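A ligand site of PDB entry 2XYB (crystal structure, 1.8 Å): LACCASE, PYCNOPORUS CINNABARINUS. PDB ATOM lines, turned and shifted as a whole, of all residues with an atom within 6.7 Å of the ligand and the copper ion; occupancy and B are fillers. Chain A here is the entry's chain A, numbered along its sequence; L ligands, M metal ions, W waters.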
ATOM      1  N   PHE A 162     -21.448  -1.720  17.751  1.00  0.00           N
ATOM      2  CA  PHE A 162     -22.275  -2.673  17.030  1.00  0.00           C
ATOM      3  C   PHE A 162     -21.541  -3.947  16.556  1.00  0.00           C
ATOM      4  O   PHE A 162     -21.054  -3.971  15.413  1.00  0.00           O
ATOM      5  CB  PHE A 162     -22.885  -2.012  15.802  1.00  0.00           C
ATOM      6  CG  PHE A 162     -23.566  -0.735  16.107  1.00  0.00           C
ATOM      7  CD1 PHE A 162     -24.736  -0.724  16.854  1.00  0.00           C
ATOM      8  CD2 PHE A 162     -22.979   0.478  15.781  1.00  0.00           C
ATOM      9  CE1 PHE A 162     -25.361   0.429  17.140  1.00  0.00           C
ATOM     10  CE2 PHE A 162     -23.607   1.652  16.042  1.00  0.00           C
ATOM     11  CZ  PHE A 162     -24.785   1.651  16.789  1.00  0.00           C
ATOM     12  N   PRO A 163     -21.517  -5.014  17.388  1.00  0.00           N
ATOM     13  CA  PRO A 163     -20.665  -6.179  17.101  1.00  0.00           C
ATOM     14  C   PRO A 163     -21.169  -6.872  15.851  1.00  0.00           C
ATOM     15  O   PRO A 163     -22.306  -6.631  15.433  1.00  0.00           O
ATOM     16  CB  PRO A 163     -20.879  -7.086  18.317  1.00  0.00           C
ATOM     17  CG  PRO A 163     -21.233  -6.087  19.411  1.00  0.00           C
ATOM     18  CD  PRO A 163     -22.114  -5.119  18.739  1.00  0.00           C
ATOM     19  N   PHE A 164     -20.254  -7.524  15.135  1.00  0.00           N
ATOM     20  CA  PHE A 164     -20.661  -8.297  13.985  1.00  0.00           C
ATOM     21  C   PHE A 164     -20.972  -9.739  14.431  1.00  0.00           C
ATOM     22  O   PHE A 164     -20.197 -10.699  14.235  1.00  0.00           O
ATOM     23  CB  PHE A 164     -19.594  -8.275  12.855  1.00  0.00           C
ATOM     24  CG  PHE A 164     -20.006  -9.069  11.676  1.00  0.00           C
ATOM     25  CD1 PHE A 164     -21.163  -8.710  10.974  1.00  0.00           C
ATOM     26  CD2 PHE A 164     -19.410 -10.289  11.412  1.00  0.00           C
ATOM     27  CE1 PHE A 164     -21.643  -9.523   9.956  1.00  0.00           C
ATOM     28  CE2 PHE A 164     -19.834 -11.054  10.370  1.00  0.00           C
ATOM     29  CZ  PHE A 164     -20.967 -10.686   9.653  1.00  0.00           C
ATOM     30  N   GLY A 165     -22.124  -9.901  15.070  1.00  0.00           N
ATOM     31  CA  GLY A 165     -22.505 -11.202  15.540  1.00  0.00           C
ATOM     32  C   GLY A 165     -21.743 -11.555  16.791  1.00  0.00           C
ATOM     33  O   GLY A 165     -20.901 -10.769  17.292  1.00  0.00           O
ATOM     34  N   ASP A 206     -29.116  -9.528  19.673  1.00  0.00           N
ATOM     35  CA  ASP A 206     -28.909  -8.906  18.361  1.00  0.00           C
ATOM     36  C   ASP A 206     -29.306  -9.839  17.199  1.00  0.00           C
ATOM     37  O   ASP A 206     -30.369  -9.662  16.627  1.00  0.00           O
ATOM     38  CB  ASP A 206     -27.441  -8.396  18.286  1.00  0.00           C
ATOM     39  CG  ASP A 206     -27.134  -7.712  16.959  1.00  0.00           C
ATOM     40  OD1 ASP A 206     -28.035  -7.662  16.082  1.00  0.00           O
ATOM     41  OD2 ASP A 206     -26.011  -7.162  16.868  1.00  0.00           O
ATOM     42  N   PRO A 207     -28.518 -10.856  16.895  1.00  0.00           N
ATOM     43  CA  PRO A 207     -28.930 -11.589  15.678  1.00  0.00           C
ATOM     44  C   PRO A 207     -30.217 -12.399  15.843  1.00  0.00           C
ATOM     45  O   PRO A 207     -30.463 -12.961  16.941  1.00  0.00           O
ATOM     46  CB  PRO A 207     -27.778 -12.584  15.461  1.00  0.00           C
ATOM     47  CG  PRO A 207     -27.154 -12.778  16.861  1.00  0.00           C
ATOM     48  CD  PRO A 207     -27.235 -11.373  17.411  1.00  0.00           C
ATOM     49  N   PHE A 265     -25.945 -13.826  11.069  1.00  0.00           N
ATOM     50  CA  PHE A 265     -24.616 -13.321  10.656  1.00  0.00           C
ATOM     51  C   PHE A 265     -23.712 -13.598  11.819  1.00  0.00           C
ATOM     52  O   PHE A 265     -24.173 -13.917  12.911  1.00  0.00           O
ATOM     53  CB  PHE A 265     -24.641 -11.781  10.371  1.00  0.00           C
ATOM     54  CG  PHE A 265     -25.369 -10.969  11.425  1.00  0.00           C
ATOM     55  CD1 PHE A 265     -24.685 -10.490  12.559  1.00  0.00           C
ATOM     56  CD2 PHE A 265     -26.720 -10.666  11.280  1.00  0.00           C
ATOM     57  CE1 PHE A 265     -25.326  -9.744  13.541  1.00  0.00           C
ATOM     58  CE2 PHE A 265     -27.393  -9.950  12.266  1.00  0.00           C
ATOM     59  CZ  PHE A 265     -26.690  -9.529  13.445  1.00  0.00           C
ATOM     60  N   PHE A 332     -30.154   7.011  10.933  1.00  0.00           N
ATOM     61  CA  PHE A 332     -28.976   6.577  11.639  1.00  0.00           C
ATOM     62  C   PHE A 332     -27.876   7.509  11.162  1.00  0.00           C
ATOM     63  O   PHE A 332     -27.874   7.882   9.996  1.00  0.00           O
ATOM     64  CB  PHE A 332     -28.642   5.173  11.212  1.00  0.00           C
ATOM     65  CG  PHE A 332     -27.393   4.616  11.819  1.00  0.00           C
ATOM     66  CD1 PHE A 332     -27.330   4.329  13.198  1.00  0.00           C
ATOM     67  CD2 PHE A 332     -26.334   4.212  11.011  1.00  0.00           C
ATOM     68  CE1 PHE A 332     -26.168   3.774  13.756  1.00  0.00           C
ATOM     69  CE2 PHE A 332     -25.192   3.576  11.558  1.00  0.00           C
ATOM     70  CZ  PHE A 332     -25.117   3.375  12.953  1.00  0.00           C
ATOM     71  N   PHE A 337     -29.186   5.809  16.356  1.00  0.00           N
ATOM     72  CA  PHE A 337     -30.424   5.693  15.575  1.00  0.00           C
ATOM     73  C   PHE A 337     -31.404   6.808  15.886  1.00  0.00           C
ATOM     74  O   PHE A 337     -31.426   7.362  17.009  1.00  0.00           O
ATOM     75  CB  PHE A 337     -31.119   4.352  15.808  1.00  0.00           C
ATOM     76  CG  PHE A 337     -30.411   3.186  15.171  1.00  0.00           C
ATOM     77  CD1 PHE A 337     -29.370   2.566  15.818  1.00  0.00           C
ATOM     78  CD2 PHE A 337     -30.770   2.771  13.902  1.00  0.00           C
ATOM     79  CE1 PHE A 337     -28.710   1.483  15.232  1.00  0.00           C
ATOM     80  CE2 PHE A 337     -30.170   1.653  13.323  1.00  0.00           C
ATOM     81  CZ  PHE A 337     -29.089   1.057  13.944  1.00  0.00           C
ATOM     82  N   ALA A 390     -31.418   2.926   7.987  1.00  0.00           N
ATOM     83  CA  ALA A 390     -31.318   2.253   9.312  1.00  0.00           C
ATOM     84  C   ALA A 390     -30.644   0.890   9.160  1.00  0.00           C
ATOM     85  O   ALA A 390     -31.325  -0.131   9.001  1.00  0.00           O
ATOM     86  CB  ALA A 390     -32.690   2.089   9.935  1.00  0.00           C
ATOM     87  N   PRO A 391     -29.303   0.875   9.131  1.00  0.00           N
ATOM     88  CA  PRO A 391     -28.579  -0.367   8.933  1.00  0.00           C
ATOM     89  C   PRO A 391     -28.770  -1.289  10.117  1.00  0.00           C
ATOM     90  O   PRO A 391     -29.298  -0.863  11.132  1.00  0.00           O
ATOM     91  CB  PRO A 391     -27.112   0.082   8.878  1.00  0.00           C
ATOM     92  CG  PRO A 391     -27.077   1.342   9.577  1.00  0.00           C
ATOM     93  CD  PRO A 391     -28.380   2.021   9.257  1.00  0.00           C
ATOM     94  N   GLY A 392     -28.357  -2.533   9.953  1.00  0.00           N
ATOM     95  CA  GLY A 392     -28.657  -3.603  10.883  1.00  0.00           C
ATOM     96  C   GLY A 392     -30.060  -4.160  10.773  1.00  0.00           C
ATOM     97  O   GLY A 392     -30.539  -4.814  11.700  1.00  0.00           O
ATOM     98  N   PHE A 393     -30.747  -3.839   9.682  1.00  0.00           N
ATOM     99  CA  PHE A 393     -32.043  -4.457   9.445  1.00  0.00           C
ATOM    100  C   PHE A 393     -31.846  -5.943   9.182  1.00  0.00           C
ATOM    101  O   PHE A 393     -30.708  -6.385   8.910  1.00  0.00           O
ATOM    102  CB  PHE A 393     -32.824  -3.717   8.354  1.00  0.00           C
ATOM    103  CG  PHE A 393     -32.128  -3.690   7.021  1.00  0.00           C
ATOM    104  CD1 PHE A 393     -32.061  -4.854   6.236  1.00  0.00           C
ATOM    105  CD2 PHE A 393     -31.470  -2.530   6.587  1.00  0.00           C
ATOM    106  CE1 PHE A 393     -31.350  -4.858   5.015  1.00  0.00           C
ATOM    107  CE2 PHE A 393     -30.725  -2.533   5.376  1.00  0.00           C
ATOM    108  CZ  PHE A 393     -30.719  -3.688   4.573  1.00  0.00           C
ATOM    109  N   PRO A 394     -32.883  -6.775   9.470  1.00  0.00           N
ATOM    110  CA  PRO A 394     -34.252  -6.400   9.855  1.00  0.00           C
ATOM    111  C   PRO A 394     -34.379  -6.130  11.384  1.00  0.00           C
ATOM    112  O   PRO A 394     -33.836  -6.877  12.197  1.00  0.00           O
ATOM    113  CB  PRO A 394     -35.088  -7.623   9.444  1.00  0.00           C
ATOM    114  CG  PRO A 394     -34.127  -8.801   9.632  1.00  0.00           C
ATOM    115  CD  PRO A 394     -32.728  -8.226   9.294  1.00  0.00           C
ATOM    116  N   HIS A 395     -34.924  -4.974  11.723  1.00  0.00           N
ATOM    117  CA  HIS A 395     -35.000  -4.564  13.130  1.00  0.00           C
ATOM    118  C   HIS A 395     -36.250  -5.198  13.723  1.00  0.00           C
ATOM    119  O   HIS A 395     -37.351  -4.862  13.305  1.00  0.00           O
ATOM    120  CB  HIS A 395     -35.130  -3.048  13.179  1.00  0.00           C
ATOM    121  CG  HIS A 395     -33.940  -2.338  12.607  1.00  0.00           C
ATOM    122  ND1 HIS A 395     -32.705  -2.353  13.230  1.00  0.00           N
ATOM    123  CD2 HIS A 395     -33.742  -1.704  11.410  1.00  0.00           C
ATOM    124  CE1 HIS A 395     -31.837  -1.690  12.496  1.00  0.00           C
ATOM    125  NE2 HIS A 395     -32.431  -1.319  11.371  1.00  0.00           N
ATOM    126  N   PRO A 396     -36.093  -5.980  14.813  1.00  0.00           N
ATOM    127  CA  PRO A 396     -37.317  -6.521  15.434  1.00  0.00           C
ATOM    128  C   PRO A 396     -37.863  -5.534  16.522  1.00  0.00           C
ATOM    129  O   PRO A 396     -37.227  -5.329  17.551  1.00  0.00           O
ATOM    130  CB  PRO A 396     -36.830  -7.833  16.069  1.00  0.00           C
ATOM    131  CG  PRO A 396     -35.391  -7.560  16.446  1.00  0.00           C
ATOM    132  CD  PRO A 396     -34.853  -6.495  15.407  1.00  0.00           C
ATOM    133  N   PHE A 397     -38.950  -4.824  16.204  1.00  0.00           N
ATOM    134  CA  PHE A 397     -39.518  -3.868  17.128  1.00  0.00           C
ATOM    135  C   PHE A 397     -40.480  -4.550  18.086  1.00  0.00           C
ATOM    136  O   PHE A 397     -41.202  -5.494  17.752  1.00  0.00           O
ATOM    137  CB  PHE A 397     -40.247  -2.694  16.376  1.00  0.00           C
ATOM    138  CG  PHE A 397     -39.350  -1.518  16.133  1.00  0.00           C
ATOM    139  CD1 PHE A 397     -38.260  -1.615  15.254  1.00  0.00           C
ATOM    140  CD2 PHE A 397     -39.501  -0.363  16.888  1.00  0.00           C
ATOM    141  CE1 PHE A 397     -37.338  -0.572  15.156  1.00  0.00           C
ATOM    142  CE2 PHE A 397     -38.660   0.713  16.700  1.00  0.00           C
ATOM    143  CZ  PHE A 397     -37.559   0.616  15.857  1.00  0.00           C
ATOM    144  N   CYS A 451     -36.461  -1.014  19.003  1.00  0.00           N
ATOM    145  CA  CYS A 451     -35.836  -2.166  18.433  1.00  0.00           C
ATOM    146  C   CYS A 451     -35.275  -3.046  19.542  1.00  0.00           C
ATOM    147  O   CYS A 451     -34.675  -2.565  20.512  1.00  0.00           O
ATOM    148  CB  CYS A 451     -34.663  -1.742  17.509  1.00  0.00           C
ATOM    149  SG  CYS A 451     -33.947  -3.221  16.825  1.00  0.00           S
ATOM    150  N   HIS A 452     -35.463  -4.349  19.427  1.00  0.00           N
ATOM    151  CA  HIS A 452     -35.019  -5.242  20.479  1.00  0.00           C
ATOM    152  C   HIS A 452     -33.614  -5.800  20.225  1.00  0.00           C
ATOM    153  O   HIS A 452     -33.134  -6.722  20.893  1.00  0.00           O
ATOM    154  CB  HIS A 452     -36.049  -6.376  20.668  1.00  0.00           C
ATOM    155  CG  HIS A 452     -36.147  -6.828  22.095  1.00  0.00           C
ATOM    156  ND1 HIS A 452     -35.060  -7.353  22.779  1.00  0.00           N
ATOM    157  CD2 HIS A 452     -37.154  -6.729  22.994  1.00  0.00           C
ATOM    158  CE1 HIS A 452     -35.449  -7.650  24.034  1.00  0.00           C
ATOM    159  NE2 HIS A 452     -36.683  -7.215  24.192  1.00  0.00           N
ATOM    160  N   ILE A 453     -32.934  -5.239  19.215  1.00  0.00           N
ATOM    161  CA  ILE A 453     -31.495  -5.415  19.144  1.00  0.00           C
ATOM    162  C   ILE A 453     -30.847  -4.461  20.166  1.00  0.00           C
ATOM    163  O   ILE A 453     -31.020  -3.272  20.088  1.00  0.00           O
ATOM    164  CB  ILE A 453     -30.967  -5.130  17.699  1.00  0.00           C
ATOM    165  CG1 ILE A 453     -31.507  -6.231  16.772  1.00  0.00           C
ATOM    166  CG2 ILE A 453     -29.440  -5.197  17.707  1.00  0.00           C
ATOM    167  CD1 ILE A 453     -31.312  -5.961  15.221  1.00  0.00           C
ATOM    168  N   PHE A 455     -28.088  -3.401  21.195  1.00  0.00           N
ATOM    169  CA  PHE A 455     -27.108  -2.387  20.768  1.00  0.00           C
ATOM    170  C   PHE A 455     -27.764  -1.206  20.075  1.00  0.00           C
ATOM    171  O   PHE A 455     -27.317  -0.059  20.254  1.00  0.00           O
ATOM    172  CB  PHE A 455     -25.994  -3.035  19.914  1.00  0.00           C
ATOM    173  CG  PHE A 455     -25.348  -4.200  20.577  1.00  0.00           C
ATOM    174  CD1 PHE A 455     -24.496  -4.043  21.686  1.00  0.00           C
ATOM    175  CD2 PHE A 455     -25.587  -5.490  20.114  1.00  0.00           C
ATOM    176  CE1 PHE A 455     -23.874  -5.146  22.274  1.00  0.00           C
ATOM    177  CE2 PHE A 455     -24.957  -6.598  20.698  1.00  0.00           C
ATOM    178  CZ  PHE A 455     -24.155  -6.450  21.802  1.00  0.00           C
ATOM    179  N   HIS A 456     -28.838  -1.453  19.337  1.00  0.00           N
ATOM    180  CA  HIS A 456     -29.572  -0.375  18.709  1.00  0.00           C
ATOM    181  C   HIS A 456     -30.388   0.440  19.713  1.00  0.00           C
ATOM    182  O   HIS A 456     -30.489   1.667  19.582  1.00  0.00           O
ATOM    183  CB  HIS A 456     -30.480  -0.896  17.572  1.00  0.00           C
ATOM    184  CG  HIS A 456     -29.733  -1.653  16.513  1.00  0.00           C
ATOM    185  ND1 HIS A 456     -30.371  -2.410  15.555  1.00  0.00           N
ATOM    186  CD2 HIS A 456     -28.406  -1.815  16.302  1.00  0.00           C
ATOM    187  CE1 HIS A 456     -29.462  -2.969  14.760  1.00  0.00           C
ATOM    188  NE2 HIS A 456     -28.271  -2.664  15.229  1.00  0.00           N
ATOM    189  N   LEU A 457     -31.135  -0.258  20.576  1.00  0.00           N
ATOM    190  CA  LEU A 457     -31.835   0.421  21.659  1.00  0.00           C
ATOM    191  C   LEU A 457     -30.884   1.383  22.368  1.00  0.00           C
ATOM    192  O   LEU A 457     -31.268   2.517  22.643  1.00  0.00           O
ATOM    193  CB  LEU A 457     -32.376  -0.623  22.675  1.00  0.00           C
ATOM    194  CG  LEU A 457     -33.030  -0.032  23.951  1.00  0.00           C
ATOM    195  CD1 LEU A 457     -34.078   1.022  23.596  1.00  0.00           C
ATOM    196  CD2 LEU A 457     -33.660  -1.183  24.840  1.00  0.00           C
ATOM    197  N   PHE A 461     -32.589   3.834  19.538  1.00  0.00           N
ATOM    198  CA  PHE A 461     -33.639   3.439  18.575  1.00  0.00           C
ATOM    199  C   PHE A 461     -34.955   3.085  19.343  1.00  0.00           C
ATOM    200  O   PHE A 461     -35.367   1.924  19.388  1.00  0.00           O
ATOM    201  CB  PHE A 461     -33.152   2.227  17.761  1.00  0.00           C
ATOM    202  CG  PHE A 461     -33.771   2.100  16.337  1.00  0.00           C
ATOM    203  CD1 PHE A 461     -34.437   3.174  15.734  1.00  0.00           C
ATOM    204  CD2 PHE A 461     -33.466   0.986  15.567  1.00  0.00           C
ATOM    205  CE1 PHE A 461     -34.940   3.074  14.453  1.00  0.00           C
ATOM    206  CE2 PHE A 461     -33.954   0.834  14.237  1.00  0.00           C
ATOM    207  CZ  PHE A 461     -34.720   1.889  13.689  1.00  0.00           C
HETATM  208  O1  LIG L   1     -24.721  -5.796  14.149  1.00  0.00           O
HETATM  209  O2  LIG L   1     -26.928  -5.617  14.049  1.00  0.00           O
HETATM  210  O3  LIG L   1     -25.894  -5.447  12.001  1.00  0.00           O
HETATM  211  C1  LIG L   1     -25.828  -1.061  12.949  1.00  0.00           C
HETATM  212  C2  LIG L   1     -25.402  -2.499  12.932  1.00  0.00           C
HETATM  213  O4  LIG L   1     -24.611  -2.872  12.108  1.00  0.00           O
HETATM  214  O5  LIG L   1     -25.925  -3.552  13.822  1.00  0.00           O
HETATM  215  S1  LIG L   1     -25.663  -5.026  13.419  1.00  0.00           S
HETATM  216 CU    CU M   1     -32.378  -2.579  15.317  1.00  0.00          CU
HETATM  217  O   HOH W   1     -23.846  -4.106   9.744  1.00  0.00           O
HETATM  218  O   HOH W   2     -29.288  -6.864  12.432  1.00  0.00           O
HETATM  219  O   HOH W   3     -22.649  -4.740  13.012  1.00  0.00           O
HETATM  220  O   HOH W   4     -26.161  -7.131   9.460  1.00  0.00           O
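Phe 162 touches the ligand (CB to C2, 3.8 Å).
Phe 265 touches the ligand.
O of Pro 391 touches C1 of the ligand (3.9 Å).
CA of Gly 392 touches O3 of the ligand, at 3.5 Å.
Hydrophobic or aromatic side chains that line the ligand: Phe 162, Phe 265 and His 456.
Along chain A the residues within 4 Å of the ligand span positions 162 to 456.
Ile 453 touches the copper ion.
Phe 461 touches the copper ion.
Of the 24 residues printed, 5 come within 4 Å of the copper ion.
The copper ion is bound by a ring nitrogen (ND1) of His 456 (2.0 Å), a ring nitrogen (ND1) of His 395 (2.1 Å) and the side-chain sulfur of Cys 451 (2.3 Å).
A ring nitrogen (NE2) of His 456 lies within hydrogen-bond range of an oxygen (O5) of the ligand (2.9 Å).
O of Pro 163 sits close to O1 of the ligand (2.9 Å).
OD1 of Asp 206 sits close to O2 of the ligand, at 3.1 Å.
Water W3 lies within hydrogen-bond range of O1 of the ligand (2.6 Å), O of Phe 162 (3.0 Å) and O of Pro 163 (3.1 Å).
Water W2 lies within hydrogen-bond range of the backbone carbonyl oxygen (O) of Gly 392 (2.5 Å) and an oxygen (O2) of the ligand (3.1 Å).
N of Phe 461 is in hydrogen-bond range of O of His 456 (3.0 Å).
The backbone carbonyl oxygen of Pro 391 sits close to a ring nitrogen (NE2) of His 395.
The backbone NH of Phe 393 sits at hydrogen-bond distance from a ring nitrogen (NE2) of His 395 (3.5 Å).
A ring nitrogen (NE2) of His 395 is in hydrogen-bond range of the backbone carbonyl oxygen (O) of Ala 390, 2.9 Å away.
The side-chain sulfur (SG) of Cys 451 sits close to the backbone NH (N) of Ile 453 (3.3 Å).
N of Cys 451 sits at hydrogen-bond distance from O of Phe 461 (3.2 Å).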
